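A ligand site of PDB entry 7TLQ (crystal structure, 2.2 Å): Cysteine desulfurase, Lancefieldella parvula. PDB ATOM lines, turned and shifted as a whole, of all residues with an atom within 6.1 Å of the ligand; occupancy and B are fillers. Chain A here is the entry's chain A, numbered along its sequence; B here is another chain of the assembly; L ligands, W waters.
Asn 120 touches the ligand. His 150 touches the ligand (CB to N1, 3.3 Å). Thr 198 touches the ligand. CB of Asn 202 touches O1 of the ligand, 3.2 Å away. Ala 229 touches the ligand. Gly 303 of chain B touches the ligand. Hydrophobic or aromatic side chains that line the ligand: His 150, Ala 229 and His 252. Along chain A the residues within 4 Å of the ligand span positions 120 to 253.
NE2 of His 252 lies within hydrogen-bond range of OG1 of Thr 304 of chain B. The side-chain amide nitrogen (ND2) of Asn 120 lies within hydrogen-bond range of the backbone carbonyl oxygen (O) of Ala 302 of chain B. The side-chain amide oxygen (OD1) of Asn 120 lies within hydrogen-bond range of the backbone NH (N) of Glu 123 (2.9 Å). O of Thr 304 of chain B sits at hydrogen-bond distance from ND2 of Asn 120 (2.8 Å). The side-chain amino group (NZ) of Lys 253 is in hydrogen-bond range of the backbone carbonyl oxygen (O) of Ala 51 (3.2 Å). The backbone carbonyl oxygen (O) of Gly 303 of chain B lies within hydrogen-bond range of the side-chain amide nitrogen (NE2) of Gln 305 of chain B (3.1 Å). NE2 of Gln 230 lies within hydrogen-bond range of O of Ala 51 (2.9 Å). The backbone NH of Ser 122 sits close to the side-chain amide oxygen of Asn 120, at 3.3 Å.
Water W1 bridges OG1 of Thr 198 (3.2 Å) and N of Asn 202 (3.5 Å).
The backbone NH (N) of Thr 121 lies within hydrogen-bond range of an oxygen (O5) of the ligand (3.4 Å). NE2 of His 252 is in hydrogen-bond range of O3 of the ligand (2.8 Å). The side-chain hydroxyl of Thr 304 of chain B is in hydrogen-bond range of an oxygen (O4) of the ligand, at 2.6 Å. An oxygen (O5) of the ligand is in hydrogen-bond range of the side-chain hydroxyl (OG) of Ser 122, at 2.6 Å. O5 of the ligand is in hydrogen-bond range of N of Ser 122, at 2.9 Å. OD2 of Asp 227 is in hydrogen-bond range of N1 of the ligand (2.6 Å). The backbone NH of Thr 304 of chain B is in hydrogen-bond range of an oxygen (O4) of the ligand. OG of Ser 250 sits at hydrogen-bond distance from O3 of the ligand. An oxygen (O1) of the ligand is in hydrogen-bond range of the side-chain amide nitrogen (NE2) of Gln 230. C5 of the ligand is covalently linked to NZ of Lys 253 (1.4 Å).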
ATOM      1  N   ALA A  51     -23.017  24.664  20.394  1.00  0.00           N
ATOM      2  CA  ALA A  51     -22.379  23.809  19.398  1.00  0.00           C
ATOM      3  C   ALA A  51     -22.112  22.417  19.952  1.00  0.00           C
ATOM      4  O   ALA A  51     -22.040  21.447  19.191  1.00  0.00           O
ATOM      5  CB  ALA A  51     -21.080  24.432  18.908  1.00  0.00           C
ATOM      6  N   ALA A  52     -21.969  22.294  21.281  1.00  0.00           N
ATOM      7  CA  ALA A  52     -21.852  20.988  21.907  1.00  0.00           C
ATOM      8  C   ALA A  52     -23.215  20.311  22.034  1.00  0.00           C
ATOM      9  O   ALA A  52     -23.411  19.201  21.544  1.00  0.00           O
ATOM     10  CB  ALA A  52     -21.175  21.118  23.272  1.00  0.00           C
ATOM     11  N   ARG A 119     -27.920   6.743  17.575  1.00  0.00           N
ATOM     12  CA  ARG A 119     -27.745   7.437  18.853  1.00  0.00           C
ATOM     13  C   ARG A 119     -27.293   8.873  18.645  1.00  0.00           C
ATOM     14  O   ARG A 119     -27.690   9.758  19.417  1.00  0.00           O
ATOM     15  CB  ARG A 119     -26.743   6.678  19.728  1.00  0.00           C
ATOM     16  CG  ARG A 119     -26.249   7.463  20.934  1.00  0.00           C
ATOM     17  CD  ARG A 119     -25.235   6.680  21.758  1.00  0.00           C
ATOM     18  NE  ARG A 119     -24.354   5.851  20.934  1.00  0.00           N
ATOM     19  CZ  ARG A 119     -24.483   4.533  20.812  1.00  0.00           C
ATOM     20  NH1 ARG A 119     -25.444   3.889  21.463  1.00  0.00           N
ATOM     21  NH2 ARG A 119     -23.636   3.854  20.044  1.00  0.00           N
ATOM     22  N   ASN A 120     -26.491   9.130  17.626  1.00  0.00           N
ATOM     23  CA  ASN A 120     -25.939  10.458  17.379  1.00  0.00           C
ATOM     24  C   ASN A 120     -25.345  10.465  15.975  1.00  0.00           C
ATOM     25  O   ASN A 120     -25.372   9.463  15.253  1.00  0.00           O
ATOM     26  CB  ASN A 120     -24.884  10.812  18.435  1.00  0.00           C
ATOM     27  CG  ASN A 120     -23.917   9.679  18.708  1.00  0.00           C
ATOM     28  OD1 ASN A 120     -23.639   8.861  17.835  1.00  0.00           O
ATOM     29  ND2 ASN A 120     -23.410   9.622  19.931  1.00  0.00           N
ATOM     30  N   THR A 121     -24.805  11.631  15.581  1.00  0.00           N
ATOM     31  CA  THR A 121     -24.122  11.737  14.291  1.00  0.00           C
ATOM     32  C   THR A 121     -22.946  10.770  14.223  1.00  0.00           C
ATOM     33  O   THR A 121     -22.665  10.200  13.160  1.00  0.00           O
ATOM     34  CB  THR A 121     -23.636  13.170  14.071  1.00  0.00           C
ATOM     35  OG1 THR A 121     -24.731  14.086  14.235  1.00  0.00           O
ATOM     36  CG2 THR A 121     -23.059  13.332  12.670  1.00  0.00           C
ATOM     37  N   SER A 122     -22.255  10.568  15.343  1.00  0.00           N
ATOM     38  CA  SER A 122     -21.082   9.709  15.367  1.00  0.00           C
ATOM     39  C   SER A 122     -21.424   8.301  14.890  1.00  0.00           C
ATOM     40  O   SER A 122     -20.716   7.738  14.042  1.00  0.00           O
ATOM     41  CB  SER A 122     -20.483   9.682  16.766  1.00  0.00           C
ATOM     42  OG  SER A 122     -20.063  10.978  17.168  1.00  0.00           O
ATOM     43  N   GLU A 123     -22.491   7.713  15.429  1.00  0.00           N
ATOM     44  CA  GLU A 123     -22.860   6.363  15.008  1.00  0.00           C
ATOM     45  C   GLU A 123     -23.308   6.343  13.558  1.00  0.00           C
ATOM     46  O   GLU A 123     -22.968   5.413  12.814  1.00  0.00           O
ATOM     47  CB  GLU A 123     -23.954   5.789  15.914  1.00  0.00           C
ATOM     48  CG  GLU A 123     -24.352   4.378  15.516  1.00  0.00           C
ATOM     49  CD  GLU A 123     -25.521   3.839  16.310  1.00  0.00           C
ATOM     50  OE1 GLU A 123     -26.249   4.647  16.929  1.00  0.00           O
ATOM     51  OE2 GLU A 123     -25.722   2.608  16.294  1.00  0.00           O
ATOM     52  N   LEU A 125     -22.272   8.168  11.135  1.00  0.00           N
ATOM     53  CA  LEU A 125     -21.099   8.225  10.278  1.00  0.00           C
ATOM     54  C   LEU A 125     -20.326   6.911  10.327  1.00  0.00           C
ATOM     55  O   LEU A 125     -19.739   6.483   9.318  1.00  0.00           O
ATOM     56  CB  LEU A 125     -20.206   9.391  10.688  1.00  0.00           C
ATOM     57  CG  LEU A 125     -20.803  10.764  10.389  1.00  0.00           C
ATOM     58  CD1 LEU A 125     -19.878  11.885  10.873  1.00  0.00           C
ATOM     59  CD2 LEU A 125     -21.096  10.922   8.903  1.00  0.00           C
ATOM     60  N   HIS A 150     -14.924  16.963  12.092  1.00  0.00           N
ATOM     61  CA  HIS A 150     -15.026  16.399  13.431  1.00  0.00           C
ATOM     62  C   HIS A 150     -14.415  15.005  13.441  1.00  0.00           C
ATOM     63  O   HIS A 150     -14.352  14.324  12.406  1.00  0.00           O
ATOM     64  CB  HIS A 150     -16.508  16.354  13.843  1.00  0.00           C
ATOM     65  CG  HIS A 150     -16.747  15.938  15.263  1.00  0.00           C
ATOM     66  ND1 HIS A 150     -16.734  14.612  15.659  1.00  0.00           N
ATOM     67  CD2 HIS A 150     -17.051  16.655  16.363  1.00  0.00           C
ATOM     68  CE1 HIS A 150     -17.006  14.542  16.953  1.00  0.00           C
ATOM     69  NE2 HIS A 150     -17.208  15.771  17.405  1.00  0.00           N
ATOM     70  N   SER A 152     -15.473  12.247  14.410  1.00  0.00           N
ATOM     71  CA  SER A 152     -16.371  11.187  13.971  1.00  0.00           C
ATOM     72  C   SER A 152     -16.481  11.096  12.452  1.00  0.00           C
ATOM     73  O   SER A 152     -16.942  10.080  11.937  1.00  0.00           O
ATOM     74  CB  SER A 152     -17.760  11.389  14.595  1.00  0.00           C
ATOM     75  OG  SER A 152     -17.701  11.233  15.997  1.00  0.00           O
ATOM     76  N   ASN A 153     -16.059  12.139  11.730  1.00  0.00           N
ATOM     77  CA  ASN A 153     -15.970  12.097  10.282  1.00  0.00           C
ATOM     78  C   ASN A 153     -14.525  11.966   9.811  1.00  0.00           C
ATOM     79  O   ASN A 153     -14.211  12.343   8.673  1.00  0.00           O
ATOM     80  CB  ASN A 153     -16.629  13.337   9.673  1.00  0.00           C
ATOM     81  CG  ASN A 153     -17.201  13.068   8.284  1.00  0.00           C
ATOM     82  OD1 ASN A 153     -17.502  11.929   7.944  1.00  0.00           O
ATOM     83  ND2 ASN A 153     -17.344  14.121   7.489  1.00  0.00           N
ATOM     84  N   THR A 198     -18.084  18.065   6.121  1.00  0.00           N
ATOM     85  CA  THR A 198     -18.979  18.740   7.045  1.00  0.00           C
ATOM     86  C   THR A 198     -19.664  19.915   6.361  1.00  0.00           C
ATOM     87  O   THR A 198     -19.057  20.632   5.555  1.00  0.00           O
ATOM     88  CB  THR A 198     -18.225  19.209   8.290  1.00  0.00           C
ATOM     89  OG1 THR A 198     -19.145  19.772   9.232  1.00  0.00           O
ATOM     90  CG2 THR A 198     -17.161  20.245   7.943  1.00  0.00           C
ATOM     91  N   VAL A 200     -21.090  22.538   8.044  1.00  0.00           N
ATOM     92  CA  VAL A 200     -20.614  23.703   8.789  1.00  0.00           C
ATOM     93  C   VAL A 200     -19.599  23.222   9.815  1.00  0.00           C
ATOM     94  O   VAL A 200     -19.839  22.240  10.528  1.00  0.00           O
ATOM     95  CB  VAL A 200     -21.772  24.462   9.477  1.00  0.00           C
ATOM     96  CG1 VAL A 200     -21.224  25.438  10.510  1.00  0.00           C
ATOM     97  CG2 VAL A 200     -22.614  25.183   8.449  1.00  0.00           C
ATOM     98  N   SER A 201     -18.450  23.902   9.880  1.00  0.00           N
ATOM     99  CA  SER A 201     -17.403  23.500  10.806  1.00  0.00           C
ATOM    100  C   SER A 201     -17.802  23.825  12.240  1.00  0.00           C
ATOM    101  O   SER A 201     -18.290  24.927  12.525  1.00  0.00           O
ATOM    102  CB  SER A 201     -16.087  24.200  10.457  1.00  0.00           C
ATOM    103  OG  SER A 201     -15.208  24.204  11.569  1.00  0.00           O
ATOM    104  N   ASN A 202     -17.578  22.883  13.147  1.00  0.00           N
ATOM    105  CA  ASN A 202     -17.907  23.061  14.559  1.00  0.00           C
ATOM    106  C   ASN A 202     -16.864  23.875  15.313  1.00  0.00           C
ATOM    107  O   ASN A 202     -17.010  24.061  16.525  1.00  0.00           O
ATOM    108  CB  ASN A 202     -18.094  21.708  15.238  1.00  0.00           C
ATOM    109  CG  ASN A 202     -16.774  21.012  15.536  1.00  0.00           C
ATOM    110  OD1 ASN A 202     -15.836  21.082  14.738  1.00  0.00           O
ATOM    111  ND2 ASN A 202     -16.708  20.339  16.672  1.00  0.00           N
ATOM    112  N   ASP A 227     -21.870  15.618   6.723  1.00  0.00           N
ATOM    113  CA  ASP A 227     -22.003  15.769   8.168  1.00  0.00           C
ATOM    114  C   ASP A 227     -22.719  17.102   8.401  1.00  0.00           C
ATOM    115  O   ASP A 227     -22.117  18.167   8.279  1.00  0.00           O
ATOM    116  CB  ASP A 227     -20.633  15.734   8.840  1.00  0.00           C
ATOM    117  CG  ASP A 227     -20.702  15.933  10.362  1.00  0.00           C
ATOM    118  OD1 ASP A 227     -21.779  16.262  10.893  1.00  0.00           O
ATOM    119  OD2 ASP A 227     -19.660  15.746  11.016  1.00  0.00           O
ATOM    120  N   ALA A 228     -24.008  17.027   8.724  1.00  0.00           N
ATOM    121  CA  ALA A 228     -24.825  18.220   8.918  1.00  0.00           C
ATOM    122  C   ALA A 228     -25.104  18.506  10.395  1.00  0.00           C
ATOM    123  O   ALA A 228     -26.087  19.182  10.715  1.00  0.00           O
ATOM    124  CB  ALA A 228     -26.151  18.079   8.153  1.00  0.00           C
ATOM    125  N   ALA A 229     -24.246  18.006  11.286  1.00  0.00           N
ATOM    126  CA  ALA A 229     -24.496  18.157  12.722  1.00  0.00           C
ATOM    127  C   ALA A 229     -24.552  19.621  13.149  1.00  0.00           C
ATOM    128  O   ALA A 229     -25.280  19.961  14.080  1.00  0.00           O
ATOM    129  CB  ALA A 229     -23.431  17.408  13.522  1.00  0.00           C
ATOM    130  N   GLN A 230     -23.798  20.490  12.474  1.00  0.00           N
ATOM    131  CA  GLN A 230     -23.768  21.907  12.812  1.00  0.00           C
ATOM    132  C   GLN A 230     -24.568  22.774  11.858  1.00  0.00           C
ATOM    133  O   GLN A 230     -24.664  23.986  12.081  1.00  0.00           O
ATOM    134  CB  GLN A 230     -22.322  22.404  12.860  1.00  0.00           C
ATOM    135  CG  GLN A 230     -21.485  21.787  13.964  1.00  0.00           C
ATOM    136  CD  GLN A 230     -21.997  22.145  15.349  1.00  0.00           C
ATOM    137  OE1 GLN A 230     -22.595  23.208  15.550  1.00  0.00           O
ATOM    138  NE2 GLN A 230     -21.751  21.280  16.316  1.00  0.00           N
ATOM    139  N   SER A 250     -27.440  15.294  14.585  1.00  0.00           N
ATOM    140  CA  SER A 250     -27.772  14.891  15.946  1.00  0.00           C
ATOM    141  C   SER A 250     -28.912  15.746  16.471  1.00  0.00           C
ATOM    142  O   SER A 250     -28.876  16.981  16.359  1.00  0.00           O
ATOM    143  CB  SER A 250     -26.555  15.002  16.874  1.00  0.00           C
ATOM    144  OG  SER A 250     -25.622  13.965  16.622  1.00  0.00           O
ATOM    145  N   HIS A 252     -29.802  16.307  19.569  1.00  0.00           N
ATOM    146  CA  HIS A 252     -29.510  17.077  20.774  1.00  0.00           C
ATOM    147  C   HIS A 252     -28.876  18.431  20.475  1.00  0.00           C
ATOM    148  O   HIS A 252     -28.810  19.274  21.373  1.00  0.00           O
ATOM    149  CB  HIS A 252     -28.607  16.273  21.717  1.00  0.00           C
ATOM    150  CG  HIS A 252     -27.207  16.106  21.226  1.00  0.00           C
ATOM    151  ND1 HIS A 252     -26.221  17.043  21.458  1.00  0.00           N
ATOM    152  CD2 HIS A 252     -26.614  15.102  20.529  1.00  0.00           C
ATOM    153  CE1 HIS A 252     -25.084  16.625  20.916  1.00  0.00           C
ATOM    154  NE2 HIS A 252     -25.308  15.456  20.344  1.00  0.00           N
ATOM    155  N   LYS A 253     -28.404  18.655  19.247  1.00  0.00           N
ATOM    156  CA  LYS A 253     -27.856  19.942  18.860  1.00  0.00           C
ATOM    157  C   LYS A 253     -28.912  20.878  18.269  1.00  0.00           C
ATOM    158  O   LYS A 253     -28.597  22.025  17.971  1.00  0.00           O
ATOM    159  CB  LYS A 253     -26.712  19.755  17.857  1.00  0.00           C
ATOM    160  CG  LYS A 253     -25.557  18.921  18.401  1.00  0.00           C
ATOM    161  CD  LYS A 253     -24.416  18.803  17.405  1.00  0.00           C
ATOM    162  CE  LYS A 253     -23.330  17.863  17.930  1.00  0.00           C
ATOM    163  NZ  LYS A 253     -21.973  18.465  17.929  1.00  0.00           N
ATOM    164  N   ARG A 408     -14.050  28.215  22.514  1.00  0.00           N
ATOM    165  CA  ARG A 408     -15.106  28.281  21.507  1.00  0.00           C
ATOM    166  C   ARG A 408     -16.391  28.758  22.163  1.00  0.00           C
ATOM    167  O   ARG A 408     -16.899  28.111  23.083  1.00  0.00           O
ATOM    168  CB  ARG A 408     -15.334  26.936  20.826  1.00  0.00           C
ATOM    169  CG  ARG A 408     -16.412  26.995  19.752  1.00  0.00           C
ATOM    170  CD  ARG A 408     -16.826  25.623  19.284  1.00  0.00           C
ATOM    171  NE  ARG A 408     -17.608  24.921  20.295  1.00  0.00           N
ATOM    172  CZ  ARG A 408     -17.914  23.625  20.237  1.00  0.00           C
ATOM    173  NH1 ARG A 408     -17.508  22.895  19.206  1.00  0.00           N
ATOM    174  NH2 ARG A 408     -18.636  23.075  21.201  1.00  0.00           N
ATOM    175  N   ALA B 302     -18.674   6.355  21.629  1.00  0.00           N
ATOM    176  CA  ALA B 302     -18.362   7.327  20.595  1.00  0.00           C
ATOM    177  C   ALA B 302     -19.454   8.390  20.536  1.00  0.00           C
ATOM    178  O   ALA B 302     -20.643   8.058  20.455  1.00  0.00           O
ATOM    179  CB  ALA B 302     -18.222   6.648  19.235  1.00  0.00           C
ATOM    180  N   GLY B 303     -19.047   9.649  20.549  1.00  0.00           N
ATOM    181  CA  GLY B 303     -19.976  10.749  20.412  1.00  0.00           C
ATOM    182  C   GLY B 303     -20.740  11.058  21.687  1.00  0.00           C
ATOM    183  O   GLY B 303     -20.506  10.480  22.753  1.00  0.00           O
ATOM    184  N   THR B 304     -21.664  11.995  21.558  1.00  0.00           N
ATOM    185  CA  THR B 304     -22.480  12.430  22.686  1.00  0.00           C
ATOM    186  C   THR B 304     -23.347  11.287  23.184  1.00  0.00           C
ATOM    187  O   THR B 304     -24.104  10.680  22.410  1.00  0.00           O
ATOM    188  CB  THR B 304     -23.346  13.619  22.288  1.00  0.00           C
ATOM    189  OG1 THR B 304     -22.513  14.675  21.778  1.00  0.00           O
ATOM    190  CG2 THR B 304     -24.148  14.126  23.473  1.00  0.00           C
ATOM    191  N   GLN B 305     -23.245  10.997  24.475  1.00  0.00           N
ATOM    192  CA  GLN B 305     -24.032   9.939  25.105  1.00  0.00           C
ATOM    193  C   GLN B 305     -25.340  10.495  25.634  1.00  0.00           C
ATOM    194  O   GLN B 305     -25.492  11.704  25.869  1.00  0.00           O
ATOM    195  CB  GLN B 305     -23.232   9.289  26.231  1.00  0.00           C
ATOM    196  CG  GLN B 305     -21.972   8.585  25.775  1.00  0.00           C
ATOM    197  CD  GLN B 305     -22.235   7.524  24.731  1.00  0.00           C
ATOM    198  OE1 GLN B 305     -22.987   6.577  24.964  1.00  0.00           O
ATOM    199  NE2 GLN B 305     -21.615   7.680  23.567  1.00  0.00           N
HETATM  200  N1  LIG L   1     -19.822  16.489  13.452  1.00  0.00           N
HETATM  201  C1  LIG L   1     -19.865  17.810  13.862  1.00  0.00           C
HETATM  202  C2  LIG L   1     -19.584  18.908  12.890  1.00  0.00           C
HETATM  203  C3  LIG L   1     -20.176  18.113  15.188  1.00  0.00           C
HETATM  204  O1  LIG L   1     -20.231  19.409  15.606  1.00  0.00           O
HETATM  205  C4  LIG L   1     -20.454  17.095  16.094  1.00  0.00           C
HETATM  206  C5  LIG L   1     -21.077  17.477  17.408  1.00  0.00           C
HETATM  207  C6  LIG L   1     -20.400  15.771  15.666  1.00  0.00           C
HETATM  208  C7  LIG L   1     -20.088  15.479  14.348  1.00  0.00           C
HETATM  209  C8  LIG L   1     -20.690  14.627  16.615  1.00  0.00           C
HETATM  210  O2  LIG L   1     -21.997  14.722  17.114  1.00  0.00           O
HETATM  211  P1  LIG L   1     -22.497  13.677  18.228  1.00  0.00           P
HETATM  212  O3  LIG L   1     -23.962  13.892  18.522  1.00  0.00           O
HETATM  213  O4  LIG L   1     -21.684  13.899  19.475  1.00  0.00           O
HETATM  214  O5  LIG L   1     -22.254  12.276  17.712  1.00  0.00           O
HETATM  215  O   HOH W   1     -16.887  19.932  11.442  1.00  0.00           O
